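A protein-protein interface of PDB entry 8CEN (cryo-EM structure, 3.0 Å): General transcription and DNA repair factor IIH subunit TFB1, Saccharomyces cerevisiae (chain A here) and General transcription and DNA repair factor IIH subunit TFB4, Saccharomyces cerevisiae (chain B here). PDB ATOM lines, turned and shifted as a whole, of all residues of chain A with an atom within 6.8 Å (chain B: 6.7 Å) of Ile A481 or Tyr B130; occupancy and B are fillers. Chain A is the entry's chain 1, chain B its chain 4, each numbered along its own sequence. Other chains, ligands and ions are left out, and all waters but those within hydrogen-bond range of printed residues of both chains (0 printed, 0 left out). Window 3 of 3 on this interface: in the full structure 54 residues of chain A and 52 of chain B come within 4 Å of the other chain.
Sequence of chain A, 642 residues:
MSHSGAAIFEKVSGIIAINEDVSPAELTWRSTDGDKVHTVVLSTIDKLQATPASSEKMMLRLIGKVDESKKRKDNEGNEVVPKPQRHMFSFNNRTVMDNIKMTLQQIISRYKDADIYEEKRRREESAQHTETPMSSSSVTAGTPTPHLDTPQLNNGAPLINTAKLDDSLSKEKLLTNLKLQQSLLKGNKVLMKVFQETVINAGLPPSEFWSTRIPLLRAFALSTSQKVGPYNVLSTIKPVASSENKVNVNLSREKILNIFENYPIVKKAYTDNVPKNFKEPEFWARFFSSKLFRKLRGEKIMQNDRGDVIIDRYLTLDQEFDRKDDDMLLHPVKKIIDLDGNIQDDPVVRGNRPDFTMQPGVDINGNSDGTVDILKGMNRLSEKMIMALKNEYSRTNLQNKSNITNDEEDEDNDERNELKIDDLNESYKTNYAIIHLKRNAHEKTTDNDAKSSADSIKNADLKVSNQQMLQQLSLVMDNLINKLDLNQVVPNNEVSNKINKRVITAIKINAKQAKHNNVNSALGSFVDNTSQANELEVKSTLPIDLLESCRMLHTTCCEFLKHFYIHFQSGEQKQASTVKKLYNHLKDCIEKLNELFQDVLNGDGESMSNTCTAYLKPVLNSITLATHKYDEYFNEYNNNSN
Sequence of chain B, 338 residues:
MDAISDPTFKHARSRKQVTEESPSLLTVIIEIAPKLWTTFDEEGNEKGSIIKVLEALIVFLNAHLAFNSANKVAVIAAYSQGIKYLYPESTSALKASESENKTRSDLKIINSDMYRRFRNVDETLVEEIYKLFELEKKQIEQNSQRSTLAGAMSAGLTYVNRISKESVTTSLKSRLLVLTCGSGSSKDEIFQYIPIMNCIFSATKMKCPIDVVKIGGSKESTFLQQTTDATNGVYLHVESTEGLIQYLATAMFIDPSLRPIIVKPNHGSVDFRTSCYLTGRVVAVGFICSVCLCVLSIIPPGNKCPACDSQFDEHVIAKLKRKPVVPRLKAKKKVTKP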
ATOM      1  N   VAL A 476     -11.179  25.296  -4.807  1.00  0.00           N
ATOM      2  CA  VAL A 476     -12.339  25.328  -5.696  1.00  0.00           C
ATOM      3  C   VAL A 476     -13.005  26.704  -5.667  1.00  0.00           C
ATOM      4  O   VAL A 476     -13.464  27.205  -6.701  1.00  0.00           O
ATOM      5  CB  VAL A 476     -13.318  24.198  -5.322  1.00  0.00           C
ATOM      6  CG1 VAL A 476     -14.607  24.295  -6.119  1.00  0.00           C
ATOM      7  CG2 VAL A 476     -12.669  22.846  -5.558  1.00  0.00           C
ATOM      8  N   MET A 477     -13.028  27.347  -4.492  1.00  0.00           N
ATOM      9  CA  MET A 477     -13.619  28.682  -4.360  1.00  0.00           C
ATOM     10  C   MET A 477     -12.893  29.688  -5.246  1.00  0.00           C
ATOM     11  O   MET A 477     -13.516  30.390  -6.056  1.00  0.00           O
ATOM     12  CB  MET A 477     -13.557  29.164  -2.905  1.00  0.00           C
ATOM     13  CG  MET A 477     -14.279  28.320  -1.868  1.00  0.00           C
ATOM     14  SD  MET A 477     -15.893  27.661  -2.291  1.00  0.00           S
ATOM     15  CE  MET A 477     -16.913  29.112  -2.132  1.00  0.00           C
ATOM     16  N   ASP A 478     -11.564  29.753  -5.119  1.00  0.00           N
ATOM     17  CA  ASP A 478     -10.811  30.735  -5.894  1.00  0.00           C
ATOM     18  C   ASP A 478     -10.796  30.380  -7.378  1.00  0.00           C
ATOM     19  O   ASP A 478     -10.829  31.276  -8.230  1.00  0.00           O
ATOM     20  CB  ASP A 478      -9.389  30.906  -5.340  1.00  0.00           C
ATOM     21  CG  ASP A 478      -8.563  29.623  -5.357  1.00  0.00           C
ATOM     22  OD1 ASP A 478      -8.307  29.054  -6.439  1.00  0.00           O
ATOM     23  OD2 ASP A 478      -8.125  29.206  -4.266  1.00  0.00           O
ATOM     24  N   ASN A 479     -10.763  29.082  -7.708  1.00  0.00           N
ATOM     25  CA  ASN A 479     -10.821  28.669  -9.106  1.00  0.00           C
ATOM     26  C   ASN A 479     -12.173  28.960  -9.739  1.00  0.00           C
ATOM     27  O   ASN A 479     -12.252  29.111 -10.963  1.00  0.00           O
ATOM     28  CB  ASN A 479     -10.500  27.179  -9.226  1.00  0.00           C
ATOM     29  CG  ASN A 479     -10.045  26.791 -10.618  1.00  0.00           C
ATOM     30  OD1 ASN A 479      -9.743  27.649 -11.447  1.00  0.00           O
ATOM     31  ND2 ASN A 479      -9.988  25.490 -10.882  1.00  0.00           N
ATOM     32  N   LEU A 480     -13.237  29.030  -8.940  1.00  0.00           N
ATOM     33  CA  LEU A 480     -14.529  29.448  -9.466  1.00  0.00           C
ATOM     34  C   LEU A 480     -14.626  30.963  -9.598  1.00  0.00           C
ATOM     35  O   LEU A 480     -15.263  31.456 -10.535  1.00  0.00           O
ATOM     36  CB  LEU A 480     -15.653  28.921  -8.574  1.00  0.00           C
ATOM     37  CG  LEU A 480     -17.019  28.722  -9.231  1.00  0.00           C
ATOM     38  CD1 LEU A 480     -16.977  27.572 -10.224  1.00  0.00           C
ATOM     39  CD2 LEU A 480     -18.085  28.480  -8.176  1.00  0.00           C
ATOM     40  N   ILE A 481     -14.014  31.714  -8.678  1.00  0.00           N
ATOM     41  CA  ILE A 481     -14.108  33.173  -8.742  1.00  0.00           C
ATOM     42  C   ILE A 481     -13.258  33.746  -9.872  1.00  0.00           C
ATOM     43  O   ILE A 481     -13.731  34.598 -10.635  1.00  0.00           O
ATOM     44  CB  ILE A 481     -13.758  33.812  -7.385  1.00  0.00           C
ATOM     45  CG1 ILE A 481     -14.742  33.337  -6.324  1.00  0.00           C
ATOM     46  CG2 ILE A 481     -13.775  35.331  -7.475  1.00  0.00           C
ATOM     47  CD1 ILE A 481     -16.161  33.746  -6.657  1.00  0.00           C
ATOM     48  N   ASN A 482     -11.996  33.306  -9.996  1.00  0.00           N
ATOM     49  CA  ASN A 482     -11.050  34.028 -10.851  1.00  0.00           C
ATOM     50  C   ASN A 482     -11.440  33.952 -12.327  1.00  0.00           C
ATOM     51  O   ASN A 482     -11.574  34.986 -12.993  1.00  0.00           O
ATOM     52  CB  ASN A 482      -9.616  33.523 -10.634  1.00  0.00           C
ATOM     53  CG  ASN A 482      -9.468  32.018 -10.812  1.00  0.00           C
ATOM     54  OD1 ASN A 482     -10.395  31.330 -11.240  1.00  0.00           O
ATOM     55  ND2 ASN A 482      -8.291  31.501 -10.479  1.00  0.00           N
ATOM     56  N   LYS A 483     -11.673  32.740 -12.838  1.00  0.00           N
ATOM     57  CA  LYS A 483     -12.125  32.525 -14.208  1.00  0.00           C
ATOM     58  C   LYS A 483     -12.585  31.086 -14.391  1.00  0.00           C
ATOM     59  O   LYS A 483     -11.869  30.148 -14.028  1.00  0.00           O
ATOM     60  CB  LYS A 483     -11.018  32.846 -15.220  1.00  0.00           C
ATOM     61  CG  LYS A 483     -11.383  32.538 -16.666  1.00  0.00           C
ATOM     62  CD  LYS A 483     -12.587  33.353 -17.124  1.00  0.00           C
ATOM     63  CE  LYS A 483     -12.277  34.842 -17.159  1.00  0.00           C
ATOM     64  NZ  LYS A 483     -13.446  35.638 -17.629  1.00  0.00           N
ATOM     65  N   LEU A 484     -13.775  30.903 -14.948  1.00  0.00           N
ATOM     66  CA  LEU A 484     -14.260  29.593 -15.367  1.00  0.00           C
ATOM     67  C   LEU A 484     -14.185  29.585 -16.891  1.00  0.00           C
ATOM     68  O   LEU A 484     -15.112  30.019 -17.576  1.00  0.00           O
ATOM     69  CB  LEU A 484     -15.675  29.331 -14.858  1.00  0.00           C
ATOM     70  CG  LEU A 484     -16.218  27.913 -15.037  1.00  0.00           C
ATOM     71  CD1 LEU A 484     -15.236  26.887 -14.494  1.00  0.00           C
ATOM     72  CD2 LEU A 484     -17.568  27.774 -14.356  1.00  0.00           C
ATOM     73  N   LEU B  86     -29.970  23.596  -8.228  1.00  0.00           N
ATOM     74  CA  LEU B  86     -28.996  24.512  -8.807  1.00  0.00           C
ATOM     75  C   LEU B  86     -29.574  25.346  -9.944  1.00  0.00           C
ATOM     76  O   LEU B  86     -29.320  26.551 -10.012  1.00  0.00           O
ATOM     77  CB  LEU B  86     -27.776  23.738  -9.313  1.00  0.00           C
ATOM     78  CG  LEU B  86     -26.992  22.936  -8.270  1.00  0.00           C
ATOM     79  CD1 LEU B  86     -25.847  22.198  -8.928  1.00  0.00           C
ATOM     80  CD2 LEU B  86     -26.486  23.807  -7.138  1.00  0.00           C
ATOM     81  N   LEU B 107     -22.808  38.186 -10.589  1.00  0.00           N
ATOM     82  CA  LEU B 107     -21.364  38.032 -10.532  1.00  0.00           C
ATOM     83  C   LEU B 107     -20.834  37.627 -11.909  1.00  0.00           C
ATOM     84  O   LEU B 107     -21.559  37.089 -12.750  1.00  0.00           O
ATOM     85  CB  LEU B 107     -20.996  37.016  -9.445  1.00  0.00           C
ATOM     86  CG  LEU B 107     -19.546  36.683  -9.092  1.00  0.00           C
ATOM     87  CD1 LEU B 107     -18.839  37.918  -8.570  1.00  0.00           C
ATOM     88  CD2 LEU B 107     -19.522  35.593  -8.041  1.00  0.00           C
ATOM     89  N   LYS B 108     -19.553  37.908 -12.143  1.00  0.00           N
ATOM     90  CA  LYS B 108     -18.960  37.845 -13.478  1.00  0.00           C
ATOM     91  C   LYS B 108     -18.123  36.590 -13.692  1.00  0.00           C
ATOM     92  O   LYS B 108     -17.058  36.653 -14.314  1.00  0.00           O
ATOM     93  CB  LYS B 108     -18.121  39.094 -13.734  1.00  0.00           C
ATOM     94  CG  LYS B 108     -18.925  40.386 -13.793  1.00  0.00           C
ATOM     95  CD  LYS B 108     -20.157  40.248 -14.674  1.00  0.00           C
ATOM     96  CE  LYS B 108     -21.090  41.435 -14.503  1.00  0.00           C
ATOM     97  NZ  LYS B 108     -20.466  42.705 -14.968  1.00  0.00           N
ATOM     98  N   ILE B 109     -18.564  35.440 -13.177  1.00  0.00           N
ATOM     99  CA  ILE B 109     -17.837  34.195 -13.410  1.00  0.00           C
ATOM    100  C   ILE B 109     -17.946  33.775 -14.873  1.00  0.00           C
ATOM    101  O   ILE B 109     -16.945  33.434 -15.515  1.00  0.00           O
ATOM    102  CB  ILE B 109     -18.341  33.092 -12.463  1.00  0.00           C
ATOM    103  CG1 ILE B 109     -18.064  33.480 -11.010  1.00  0.00           C
ATOM    104  CG2 ILE B 109     -17.691  31.759 -12.795  1.00  0.00           C
ATOM    105  CD1 ILE B 109     -18.744  32.593 -10.000  1.00  0.00           C
ATOM    106  N   LEU B 125     -26.549  28.389 -12.356  1.00  0.00           N
ATOM    107  CA  LEU B 125     -25.891  27.164 -11.912  1.00  0.00           C
ATOM    108  C   LEU B 125     -24.630  27.464 -11.105  1.00  0.00           C
ATOM    109  O   LEU B 125     -24.437  26.917 -10.012  1.00  0.00           O
ATOM    110  CB  LEU B 125     -25.568  26.299 -13.129  1.00  0.00           C
ATOM    111  CG  LEU B 125     -25.069  24.875 -12.913  1.00  0.00           C
ATOM    112  CD1 LEU B 125     -25.734  23.953 -13.902  1.00  0.00           C
ATOM    113  CD2 LEU B 125     -23.576  24.830 -13.099  1.00  0.00           C
ATOM    114  N   VAL B 126     -23.766  28.346 -11.617  1.00  0.00           N
ATOM    115  CA  VAL B 126     -22.505  28.615 -10.925  1.00  0.00           C
ATOM    116  C   VAL B 126     -22.727  29.418  -9.640  1.00  0.00           C
ATOM    117  O   VAL B 126     -22.030  29.193  -8.640  1.00  0.00           O
ATOM    118  CB  VAL B 126     -21.498  29.296 -11.872  1.00  0.00           C
ATOM    119  CG1 VAL B 126     -20.152  29.435 -11.206  1.00  0.00           C
ATOM    120  CG2 VAL B 126     -21.306  28.457 -13.111  1.00  0.00           C
ATOM    121  N   GLU B 127     -23.695  30.344  -9.623  1.00  0.00           N
ATOM    122  CA  GLU B 127     -24.007  31.045  -8.379  1.00  0.00           C
ATOM    123  C   GLU B 127     -24.552  30.097  -7.319  1.00  0.00           C
ATOM    124  O   GLU B 127     -24.219  30.230  -6.136  1.00  0.00           O
ATOM    125  CB  GLU B 127     -25.000  32.185  -8.616  1.00  0.00           C
ATOM    126  CG  GLU B 127     -24.474  33.354  -9.424  1.00  0.00           C
ATOM    127  CD  GLU B 127     -25.529  34.427  -9.623  1.00  0.00           C
ATOM    128  OE1 GLU B 127     -26.693  34.190  -9.236  1.00  0.00           O
ATOM    129  OE2 GLU B 127     -25.199  35.505 -10.156  1.00  0.00           O
ATOM    130  N   GLU B 128     -25.387  29.130  -7.715  1.00  0.00           N
ATOM    131  CA  GLU B 128     -25.868  28.168  -6.729  1.00  0.00           C
ATOM    132  C   GLU B 128     -24.761  27.219  -6.274  1.00  0.00           C
ATOM    133  O   GLU B 128     -24.760  26.797  -5.112  1.00  0.00           O
ATOM    134  CB  GLU B 128     -27.063  27.398  -7.283  1.00  0.00           C
ATOM    135  CG  GLU B 128     -28.317  28.245  -7.424  1.00  0.00           C
ATOM    136  CD  GLU B 128     -28.691  28.951  -6.136  1.00  0.00           C
ATOM    137  OE1 GLU B 128     -28.842  28.266  -5.103  1.00  0.00           O
ATOM    138  OE2 GLU B 128     -28.836  30.191  -6.157  1.00  0.00           O
ATOM    139  N   ILE B 129     -23.811  26.891  -7.156  1.00  0.00           N
ATOM    140  CA  ILE B 129     -22.620  26.141  -6.745  1.00  0.00           C
ATOM    141  C   ILE B 129     -21.828  26.915  -5.696  1.00  0.00           C
ATOM    142  O   ILE B 129     -21.412  26.361  -4.668  1.00  0.00           O
ATOM    143  CB  ILE B 129     -21.751  25.800  -7.971  1.00  0.00           C
ATOM    144  CG1 ILE B 129     -22.407  24.713  -8.821  1.00  0.00           C
ATOM    145  CG2 ILE B 129     -20.351  25.379  -7.561  1.00  0.00           C
ATOM    146  CD1 ILE B 129     -22.479  23.379  -8.122  1.00  0.00           C
ATOM    147  N   TYR B 130     -21.617  28.213  -5.940  1.00  0.00           N
ATOM    148  CA  TYR B 130     -20.886  29.052  -4.992  1.00  0.00           C
ATOM    149  C   TYR B 130     -21.614  29.157  -3.657  1.00  0.00           C
ATOM    150  O   TYR B 130     -20.987  29.076  -2.594  1.00  0.00           O
ATOM    151  CB  TYR B 130     -20.664  30.442  -5.591  1.00  0.00           C
ATOM    152  CG  TYR B 130     -19.763  31.331  -4.765  1.00  0.00           C
ATOM    153  CD1 TYR B 130     -18.387  31.157  -4.766  1.00  0.00           C
ATOM    154  CD2 TYR B 130     -20.295  32.349  -3.982  1.00  0.00           C
ATOM    155  CE1 TYR B 130     -17.567  31.973  -4.008  1.00  0.00           C
ATOM    156  CE2 TYR B 130     -19.480  33.168  -3.222  1.00  0.00           C
ATOM    157  CZ  TYR B 130     -18.117  32.974  -3.240  1.00  0.00           C
ATOM    158  OH  TYR B 130     -17.300  33.785  -2.487  1.00  0.00           O
ATOM    159  N   LYS B 131     -22.938  29.331  -3.694  1.00  0.00           N
ATOM    160  CA  LYS B 131     -23.715  29.418  -2.462  1.00  0.00           C
ATOM    161  C   LYS B 131     -23.690  28.105  -1.688  1.00  0.00           C
ATOM    162  O   LYS B 131     -23.580  28.109  -0.457  1.00  0.00           O
ATOM    163  CB  LYS B 131     -25.154  29.828  -2.774  1.00  0.00           C
ATOM    164  CG  LYS B 131     -25.305  31.274  -3.207  1.00  0.00           C
ATOM    165  CD  LYS B 131     -26.756  31.610  -3.490  1.00  0.00           C
ATOM    166  CE  LYS B 131     -26.913  33.053  -3.935  1.00  0.00           C
ATOM    167  NZ  LYS B 131     -28.334  33.381  -4.230  1.00  0.00           N
ATOM    168  N   LEU B 132     -23.785  26.972  -2.392  1.00  0.00           N
ATOM    169  CA  LEU B 132     -23.741  25.673  -1.730  1.00  0.00           C
ATOM    170  C   LEU B 132     -22.383  25.421  -1.086  1.00  0.00           C
ATOM    171  O   LEU B 132     -22.311  24.942   0.054  1.00  0.00           O
ATOM    172  CB  LEU B 132     -24.074  24.569  -2.736  1.00  0.00           C
ATOM    173  CG  LEU B 132     -24.418  23.178  -2.201  1.00  0.00           C
ATOM    174  CD1 LEU B 132     -25.536  22.575  -3.025  1.00  0.00           C
ATOM    175  CD2 LEU B 132     -23.204  22.269  -2.214  1.00  0.00           C
ATOM    176  N   PHE B 133     -21.297  25.735  -1.800  1.00  0.00           N
ATOM    177  CA  PHE B 133     -19.966  25.561  -1.228  1.00  0.00           C
ATOM    178  C   PHE B 133     -19.722  26.502  -0.056  1.00  0.00           C
ATOM    179  O   PHE B 133     -19.078  26.113   0.922  1.00  0.00           O
ATOM    180  CB  PHE B 133     -18.887  25.732  -2.296  1.00  0.00           C
ATOM    181  CG  PHE B 133     -18.836  24.617  -3.304  1.00  0.00           C
ATOM    182  CD1 PHE B 133     -19.481  23.416  -3.061  1.00  0.00           C
ATOM    183  CD2 PHE B 133     -18.118  24.759  -4.478  1.00  0.00           C
ATOM    184  CE1 PHE B 133     -19.421  22.387  -3.973  1.00  0.00           C
ATOM    185  CE2 PHE B 133     -18.058  23.728  -5.397  1.00  0.00           C
ATOM    186  CZ  PHE B 133     -18.713  22.544  -5.145  1.00  0.00           C
ATOM    187  N   GLU B 134     -20.236  27.734  -0.120  1.00  0.00           N
ATOM    188  CA  GLU B 134     -20.107  28.640   1.017  1.00  0.00           C
ATOM    189  C   GLU B 134     -20.904  28.140   2.219  1.00  0.00           C
ATOM    190  O   GLU B 134     -20.436  28.222   3.363  1.00  0.00           O
ATOM    191  CB  GLU B 134     -20.552  30.049   0.621  1.00  0.00           C
ATOM    192  CG  GLU B 134     -20.474  31.074   1.746  1.00  0.00           C
ATOM    193  CD  GLU B 134     -19.048  31.384   2.165  1.00  0.00           C
ATOM    194  OE1 GLU B 134     -18.135  31.271   1.320  1.00  0.00           O
ATOM    195  OE2 GLU B 134     -18.840  31.741   3.344  1.00  0.00           O
ATOM    196  N   LEU B 135     -22.103  27.597   1.975  1.00  0.00           N
ATOM    197  CA  LEU B 135     -22.924  27.066   3.058  1.00  0.00           C
ATOM    198  C   LEU B 135     -22.260  25.870   3.730  1.00  0.00           C
ATOM    199  O   LEU B 135     -22.222  25.787   4.964  1.00  0.00           O
ATOM    200  CB  LEU B 135     -24.308  26.688   2.522  1.00  0.00           C
ATOM    201  CG  LEU B 135     -25.353  26.091   3.471  1.00  0.00           C
ATOM    202  CD1 LEU B 135     -26.702  26.749   3.242  1.00  0.00           C
ATOM    203  CD2 LEU B 135     -25.470  24.587   3.265  1.00  0.00           C
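Among the printed residues, pairs that only touch across the chains: Leu A480 with Ile B109, Met A477 with Tyr B130, Ile A481 with Tyr B130, Met A477 with Phe B133, Val A476 with Phe B133, Leu A484 with Ile B109, Leu A480 with Val B126, Leu A480 with Ile B129 and Leu A484 with Val B126.
Of the printed residues of chain B, Ile A481 touches Tyr B130.
Tyr B130 touches just these residues of chain A: Met A477 (3.5 Å) and Ile A481 (3.5 Å).
Printed residues of chain B within 4 Å of Leu A484: Ile B109 (3.8 Å) and Val B126 (3.999 Å).
Of the printed residues of chain A, Phe B133 touches Val A476 (3.6 Å) and Met A477 (3.6 Å).
Printed residues of chain A within 4 Å of Ile B109: Leu A480 (3.3 Å) and Leu A484 (3.8 Å).
The nearest printed residue of chain A that does not touch Val B126 is Ile A481 (7.0 Å).
Of the 9 printed residues of chain A, 5 touch a printed residue of chain B.
Hydrophobic or aromatic side chains of chain A that line the printed part of chain B: Val A476, Met A477, Leu A480, Ile A481 and Leu A484.
Of the 15 printed residues of chain B, 5 touch a printed residue of chain A.
Along chain B the printed residues that touch a printed residue of chain A span positions 109 to 133.
Among the printed residues, no Asp or Glu carboxylate lies within 4 Å of a Lys or Arg side-chain nitrogen of the other chain.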
